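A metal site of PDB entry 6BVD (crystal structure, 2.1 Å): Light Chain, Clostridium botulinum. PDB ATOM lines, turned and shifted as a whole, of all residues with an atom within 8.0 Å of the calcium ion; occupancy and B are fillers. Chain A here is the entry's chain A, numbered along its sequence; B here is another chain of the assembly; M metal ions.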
ATOM      1  N   LYS A  95      25.549  33.506  20.743  1.00  0.00           N
ATOM      2  CA  LYS A  95      25.222  33.685  22.176  1.00  0.00           C
ATOM      3  C   LYS A  95      24.198  34.810  22.371  1.00  0.00           C
ATOM      4  O   LYS A  95      23.251  34.708  23.184  1.00  0.00           O
ATOM      5  CB  LYS A  95      26.494  33.954  22.975  1.00  0.00           C
ATOM      6  CG  LYS A  95      26.301  33.795  24.506  1.00  0.00           C
ATOM      7  CD  LYS A  95      27.624  33.824  25.244  1.00  0.00           C
ATOM      8  CE  LYS A  95      27.359  33.617  26.758  1.00  0.00           C
ATOM      9  NZ  LYS A  95      28.629  33.199  27.358  1.00  0.00           N
ATOM     10  N   LYS A  98      20.749  33.650  21.246  1.00  0.00           N
ATOM     11  CA  LYS A  98      20.204  32.761  22.278  1.00  0.00           C
ATOM     12  C   LYS A  98      19.753  33.552  23.517  1.00  0.00           C
ATOM     13  O   LYS A  98      18.809  33.155  24.184  1.00  0.00           O
ATOM     14  CB  LYS A  98      21.198  31.669  22.697  1.00  0.00           C
ATOM     15  CG  LYS A  98      21.331  30.554  21.629  1.00  0.00           C
ATOM     16  CD  LYS A  98      22.019  29.274  22.110  1.00  0.00           C
ATOM     17  CE  LYS A  98      23.537  29.322  21.994  1.00  0.00           C
ATOM     18  NZ  LYS A  98      24.257  28.036  22.248  1.00  0.00           N
ATOM     19  N   LEU A 381      32.873  37.790  26.497  1.00  0.00           N
ATOM     20  CA  LEU A 381      31.448  37.580  26.376  1.00  0.00           C
ATOM     21  C   LEU A 381      31.138  36.071  26.297  1.00  0.00           C
ATOM     22  O   LEU A 381      30.049  35.624  26.688  1.00  0.00           O
ATOM     23  CB  LEU A 381      30.889  38.320  25.153  1.00  0.00           C
ATOM     24  CG  LEU A 381      30.956  39.873  25.241  1.00  0.00           C
ATOM     25  CD1 LEU A 381      30.518  40.520  23.930  1.00  0.00           C
ATOM     26  CD2 LEU A 381      30.087  40.364  26.396  1.00  0.00           C
ATOM     27  N   LEU A 382      32.102  35.320  25.785  1.00  0.00           N
ATOM     28  CA  LEU A 382      31.911  33.874  25.604  1.00  0.00           C
ATOM     29  C   LEU A 382      32.065  33.054  26.882  1.00  0.00           C
ATOM     30  O   LEU A 382      31.678  31.891  26.910  1.00  0.00           O
ATOM     31  CB  LEU A 382      32.905  33.338  24.559  1.00  0.00           C
ATOM     32  CG  LEU A 382      32.601  33.723  23.108  1.00  0.00           C
ATOM     33  CD1 LEU A 382      33.785  33.318  22.259  1.00  0.00           C
ATOM     34  CD2 LEU A 382      31.384  32.974  22.690  1.00  0.00           C
ATOM     35  N   ASP A 383      32.622  33.665  27.940  1.00  0.00           N
ATOM     36  CA  ASP A 383      32.854  33.023  29.240  1.00  0.00           C
ATOM     37  C   ASP A 383      31.624  33.095  30.153  1.00  0.00           C
ATOM     38  O   ASP A 383      31.264  34.176  30.635  1.00  0.00           O
ATOM     39  CB  ASP A 383      34.077  33.693  29.911  1.00  0.00           C
ATOM     40  CG  ASP A 383      34.549  32.987  31.192  1.00  0.00           C
ATOM     41  OD1 ASP A 383      33.764  32.312  31.891  1.00  0.00           O
ATOM     42  OD2 ASP A 383      35.733  33.157  31.530  1.00  0.00           O
ATOM     43  N   ASP A 384      31.010  31.940  30.438  1.00  0.00           N
ATOM     44  CA  ASP A 384      29.744  31.897  31.186  1.00  0.00           C
ATOM     45  C   ASP A 384      29.907  32.328  32.653  1.00  0.00           C
ATOM     46  O   ASP A 384      28.897  32.527  33.336  1.00  0.00           O
ATOM     47  CB  ASP A 384      29.123  30.491  31.109  1.00  0.00           C
ATOM     48  CG  ASP A 384      28.362  30.258  29.774  1.00  0.00           C
ATOM     49  OD1 ASP A 384      27.590  31.137  29.367  1.00  0.00           O
ATOM     50  OD2 ASP A 384      28.591  29.229  29.115  1.00  0.00           O
ATOM     51  N   SER A 385      31.139  32.442  33.156  1.00  0.00           N
ATOM     52  CA  SER A 385      31.318  33.050  34.485  1.00  0.00           C
ATOM     53  C   SER A 385      31.311  34.589  34.458  1.00  0.00           C
ATOM     54  O   SER A 385      31.300  35.234  35.521  1.00  0.00           O
ATOM     55  CB  SER A 385      32.627  32.573  35.129  1.00  0.00           C
ATOM     56  OG  SER A 385      33.768  33.043  34.453  1.00  0.00           O
ATOM     57  N   TYR A 387      29.526  36.428  31.464  1.00  0.00           N
ATOM     58  CA  TYR A 387      28.348  36.816  30.741  1.00  0.00           C
ATOM     59  C   TYR A 387      27.572  35.547  30.341  1.00  0.00           C
ATOM     60  O   TYR A 387      28.165  34.655  29.743  1.00  0.00           O
ATOM     61  CB  TYR A 387      28.767  37.615  29.499  1.00  0.00           C
ATOM     62  CG  TYR A 387      27.631  38.152  28.684  1.00  0.00           C
ATOM     63  CD1 TYR A 387      27.071  39.381  28.980  1.00  0.00           C
ATOM     64  CD2 TYR A 387      27.169  37.473  27.542  1.00  0.00           C
ATOM     65  CE1 TYR A 387      26.052  39.897  28.233  1.00  0.00           C
ATOM     66  CE2 TYR A 387      26.127  38.005  26.771  1.00  0.00           C
ATOM     67  CZ  TYR A 387      25.586  39.221  27.114  1.00  0.00           C
ATOM     68  OH  TYR A 387      24.574  39.798  26.348  1.00  0.00           O
ATOM     69  N   THR A 388      26.295  35.455  30.668  1.00  0.00           N
ATOM     70  CA  THR A 388      25.522  34.257  30.279  1.00  0.00           C
ATOM     71  C   THR A 388      24.362  34.548  29.355  1.00  0.00           C
ATOM     72  O   THR A 388      23.811  35.671  29.322  1.00  0.00           O
ATOM     73  CB  THR A 388      24.923  33.518  31.496  1.00  0.00           C
ATOM     74  OG1 THR A 388      23.980  34.371  32.182  1.00  0.00           O
ATOM     75  CG2 THR A 388      26.031  33.046  32.424  1.00  0.00           C
ATOM     76  N   GLU A 389      23.923  33.527  28.593  1.00  0.00           N
ATOM     77  CA  GLU A 389      22.669  33.675  27.817  1.00  0.00           C
ATOM     78  C   GLU A 389      21.480  34.141  28.659  1.00  0.00           C
ATOM     79  O   GLU A 389      20.739  35.027  28.260  1.00  0.00           O
ATOM     80  CB  GLU A 389      22.259  32.326  27.167  1.00  0.00           C
ATOM     81  CG  GLU A 389      23.232  31.829  26.057  1.00  0.00           C
ATOM     82  CD  GLU A 389      24.420  31.014  26.556  1.00  0.00           C
ATOM     83  OE1 GLU A 389      24.635  30.797  27.799  1.00  0.00           O
ATOM     84  OE2 GLU A 389      25.202  30.585  25.698  1.00  0.00           O
ATOM     85  N   VAL A 390      21.264  33.499  29.797  1.00  0.00           N
ATOM     86  CA  VAL A 390      20.035  33.704  30.591  1.00  0.00           C
ATOM     87  C   VAL A 390      20.082  35.032  31.366  1.00  0.00           C
ATOM     88  O   VAL A 390      19.020  35.667  31.552  1.00  0.00           O
ATOM     89  CB  VAL A 390      19.773  32.494  31.566  1.00  0.00           C
ATOM     90  CG1 VAL A 390      20.907  32.300  32.579  1.00  0.00           C
ATOM     91  CG2 VAL A 390      18.422  32.616  32.304  1.00  0.00           C
ATOM     92  N   LYS B  95      26.645  25.236  34.519  1.00  0.00           N
ATOM     93  CA  LYS B  95      26.584  24.950  33.075  1.00  0.00           C
ATOM     94  C   LYS B  95      26.211  23.474  32.774  1.00  0.00           C
ATOM     95  O   LYS B  95      25.445  23.219  31.861  1.00  0.00           O
ATOM     96  CB  LYS B  95      27.912  25.312  32.434  1.00  0.00           C
ATOM     97  CG  LYS B  95      27.821  25.396  30.884  1.00  0.00           C
ATOM     98  CD  LYS B  95      29.061  26.072  30.262  1.00  0.00           C
ATOM     99  CE  LYS B  95      28.904  26.215  28.743  1.00  0.00           C
ATOM    100  NZ  LYS B  95      29.848  27.224  28.205  1.00  0.00           N
ATOM    101  N   LYS B  98      22.553  23.028  33.418  1.00  0.00           N
ATOM    102  CA  LYS B  98      21.758  23.613  32.360  1.00  0.00           C
ATOM    103  C   LYS B  98      21.800  22.686  31.130  1.00  0.00           C
ATOM    104  O   LYS B  98      20.791  22.548  30.419  1.00  0.00           O
ATOM    105  CB  LYS B  98      22.210  25.035  31.989  1.00  0.00           C
ATOM    106  CG  LYS B  98      21.758  26.118  33.044  1.00  0.00           C
ATOM    107  CD  LYS B  98      21.861  27.581  32.584  1.00  0.00           C
ATOM    108  CE  LYS B  98      23.219  28.251  32.890  1.00  0.00           C
ATOM    109  NZ  LYS B  98      23.262  29.743  32.604  1.00  0.00           N
ATOM    110  N   LEU B 381      35.716  24.747  29.683  1.00  0.00           N
ATOM    111  CA  LEU B 381      34.328  24.335  29.621  1.00  0.00           C
ATOM    112  C   LEU B 381      33.400  25.548  29.646  1.00  0.00           C
ATOM    113  O   LEU B 381      32.341  25.527  29.058  1.00  0.00           O
ATOM    114  CB  LEU B 381      34.001  23.366  30.779  1.00  0.00           C
ATOM    115  CG  LEU B 381      34.730  22.008  30.752  1.00  0.00           C
ATOM    116  CD1 LEU B 381      34.519  21.203  32.042  1.00  0.00           C
ATOM    117  CD2 LEU B 381      34.238  21.193  29.546  1.00  0.00           C
ATOM    118  N   LEU B 382      33.830  26.633  30.312  1.00  0.00           N
ATOM    119  CA  LEU B 382      32.990  27.838  30.408  1.00  0.00           C
ATOM    120  C   LEU B 382      32.984  28.686  29.103  1.00  0.00           C
ATOM    121  O   LEU B 382      32.184  29.573  28.947  1.00  0.00           O
ATOM    122  CB  LEU B 382      33.470  28.706  31.575  1.00  0.00           C
ATOM    123  CG  LEU B 382      33.154  28.128  32.970  1.00  0.00           C
ATOM    124  CD1 LEU B 382      33.924  28.967  34.009  1.00  0.00           C
ATOM    125  CD2 LEU B 382      31.672  28.209  33.216  1.00  0.00           C
ATOM    126  N   ASP B 383      33.870  28.364  28.160  1.00  0.00           N
ATOM    127  CA  ASP B 383      33.970  29.100  26.878  1.00  0.00           C
ATOM    128  C   ASP B 383      32.986  28.553  25.833  1.00  0.00           C
ATOM    129  O   ASP B 383      33.135  27.409  25.388  1.00  0.00           O
ATOM    130  CB  ASP B 383      35.398  28.996  26.351  1.00  0.00           C
ATOM    131  CG  ASP B 383      35.662  29.897  25.117  1.00  0.00           C
ATOM    132  OD1 ASP B 383      34.732  30.244  24.358  1.00  0.00           O
ATOM    133  OD2 ASP B 383      36.834  30.215  24.895  1.00  0.00           O
ATOM    134  N   ASP B 384      31.995  29.334  25.463  1.00  0.00           N
ATOM    135  CA  ASP B 384      30.929  28.839  24.575  1.00  0.00           C
ATOM    136  C   ASP B 384      31.423  28.575  23.146  1.00  0.00           C
ATOM    137  O   ASP B 384      30.683  27.996  22.366  1.00  0.00           O
ATOM    138  CB  ASP B 384      29.754  29.821  24.522  1.00  0.00           C
ATOM    139  CG  ASP B 384      28.773  29.685  25.726  1.00  0.00           C
ATOM    140  OD1 ASP B 384      28.382  28.568  26.091  1.00  0.00           O
ATOM    141  OD2 ASP B 384      28.317  30.715  26.266  1.00  0.00           O
ATOM    142  N   SER B 385      32.650  28.985  22.811  1.00  0.00           N
ATOM    143  CA  SER B 385      33.209  28.670  21.471  1.00  0.00           C
ATOM    144  C   SER B 385      33.828  27.267  21.522  1.00  0.00           C
ATOM    145  O   SER B 385      34.243  26.723  20.487  1.00  0.00           O
ATOM    146  CB  SER B 385      34.263  29.704  21.042  1.00  0.00           C
ATOM    147  OG  SER B 385      35.425  29.633  21.845  1.00  0.00           O
ATOM    148  N   TYR B 387      32.566  24.717  24.301  1.00  0.00           N
ATOM    149  CA  TYR B 387      31.614  23.807  24.940  1.00  0.00           C
ATOM    150  C   TYR B 387      30.343  24.588  25.297  1.00  0.00           C
ATOM    151  O   TYR B 387      30.421  25.618  25.991  1.00  0.00           O
ATOM    152  CB  TYR B 387      32.260  23.192  26.187  1.00  0.00           C
ATOM    153  CG  TYR B 387      31.432  22.162  26.903  1.00  0.00           C
ATOM    154  CD1 TYR B 387      31.472  20.828  26.529  1.00  0.00           C
ATOM    155  CD2 TYR B 387      30.604  22.529  27.976  1.00  0.00           C
ATOM    156  CE1 TYR B 387      30.699  19.874  27.218  1.00  0.00           C
ATOM    157  CE2 TYR B 387      29.846  21.583  28.648  1.00  0.00           C
ATOM    158  CZ  TYR B 387      29.876  20.251  28.271  1.00  0.00           C
ATOM    159  OH  TYR B 387      29.115  19.302  28.957  1.00  0.00           O
ATOM    160  N   THR B 388      29.186  24.166  24.795  1.00  0.00           N
ATOM    161  CA  THR B 388      27.934  24.886  25.037  1.00  0.00           C
ATOM    162  C   THR B 388      26.972  24.033  25.845  1.00  0.00           C
ATOM    163  O   THR B 388      27.125  22.797  25.907  1.00  0.00           O
ATOM    164  CB  THR B 388      27.208  25.291  23.741  1.00  0.00           C
ATOM    165  OG1 THR B 388      26.985  24.115  22.925  1.00  0.00           O
ATOM    166  CG2 THR B 388      28.033  26.336  22.952  1.00  0.00           C
ATOM    167  N   GLU B 389      26.038  24.721  26.501  1.00  0.00           N
ATOM    168  CA  GLU B 389      24.931  24.049  27.199  1.00  0.00           C
ATOM    169  C   GLU B 389      24.173  23.125  26.208  1.00  0.00           C
ATOM    170  O   GLU B 389      23.834  21.976  26.536  1.00  0.00           O
ATOM    171  CB  GLU B 389      23.971  25.081  27.805  1.00  0.00           C
ATOM    172  CG  GLU B 389      24.606  25.951  28.928  1.00  0.00           C
ATOM    173  CD  GLU B 389      25.314  27.240  28.428  1.00  0.00           C
ATOM    174  OE1 GLU B 389      25.418  27.471  27.173  1.00  0.00           O
ATOM    175  OE2 GLU B 389      25.786  28.049  29.305  1.00  0.00           O
ATOM    176  N   VAL B 390      23.891  23.651  25.026  1.00  0.00           N
ATOM    177  CA  VAL B 390      23.004  22.966  24.070  1.00  0.00           C
ATOM    178  C   VAL B 390      23.695  21.796  23.344  1.00  0.00           C
ATOM    179  O   VAL B 390      23.042  20.752  23.057  1.00  0.00           O
ATOM    180  CB  VAL B 390      22.454  23.987  23.017  1.00  0.00           C
ATOM    181  CG1 VAL B 390      23.584  24.605  22.199  1.00  0.00           C
ATOM    182  CG2 VAL B 390      21.442  23.333  22.096  1.00  0.00           C
HETATM  183 CA    CA M   1      26.795  29.522  27.714  1.00  0.00          CA
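OD2 of Asp 384 of chain A lies close to NZ of Lys 95 of chain B, 2.5 Å away.
The side-chain carboxylate of Asp 384 of chain A lies close to the side-chain amino group of Lys 95 of chain A (3.1 Å).
O of Leu 382 of chain B is in hydrogen-bond range of N of Asp 384 of chain A, at 3.0 Å.
The side-chain amino group (NZ) of Lys 95 of chain B sits close to the side-chain carboxylate (OD1) of Asp 384 of chain B (2.9 Å).
The side-chain amino group (NZ) of Lys 95 of chain A lies close to the side-chain carboxylate (OD2) of Asp 384 of chain B (2.7 Å).
NZ of Lys 95 of chain B is in hydrogen-bond range of O of Leu 382 of chain B, at 3.4 Å.
The backbone carbonyl oxygen of Tyr 387 of chain B is in hydrogen-bond range of the side-chain amino group of Lys 95 of chain B (2.8 Å).
The side-chain amino group (NZ) of Lys 95 of chain B sits at hydrogen-bond distance from the backbone carbonyl oxygen (O) of Leu 381 of chain B.
Merely in contact with the calcium ion: Lys 95 of chain B (3.9 Å).
The calcium ion is bound by OD2 of Asp 384 of chain A (2.3 Å).
The side-chain carboxylate (OE2) of Glu 389 of chain B is bound to the calcium ion, 2.4 Å away.
The calcium ion is bound by OD2 of Asp 384 of chain B (2.4 Å).
OD1 of Asp 384 of chain A binds the calcium ion, 2.4 Å away.
The side-chain carboxylate (OD1) of Asp 384 of chain B is bound to the calcium ion (2.5 Å).
The calcium ion is bound by OE1 of Glu 389 of chain A, at 2.5 Å.
The calcium ion is bound by OE1 of Glu 389 of chain B (2.5 Å).
The calcium ion is bound by the side-chain carboxylate (OE2) of Glu 389 of chain A.
The calcium ion has eight donor atoms within binding distance.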
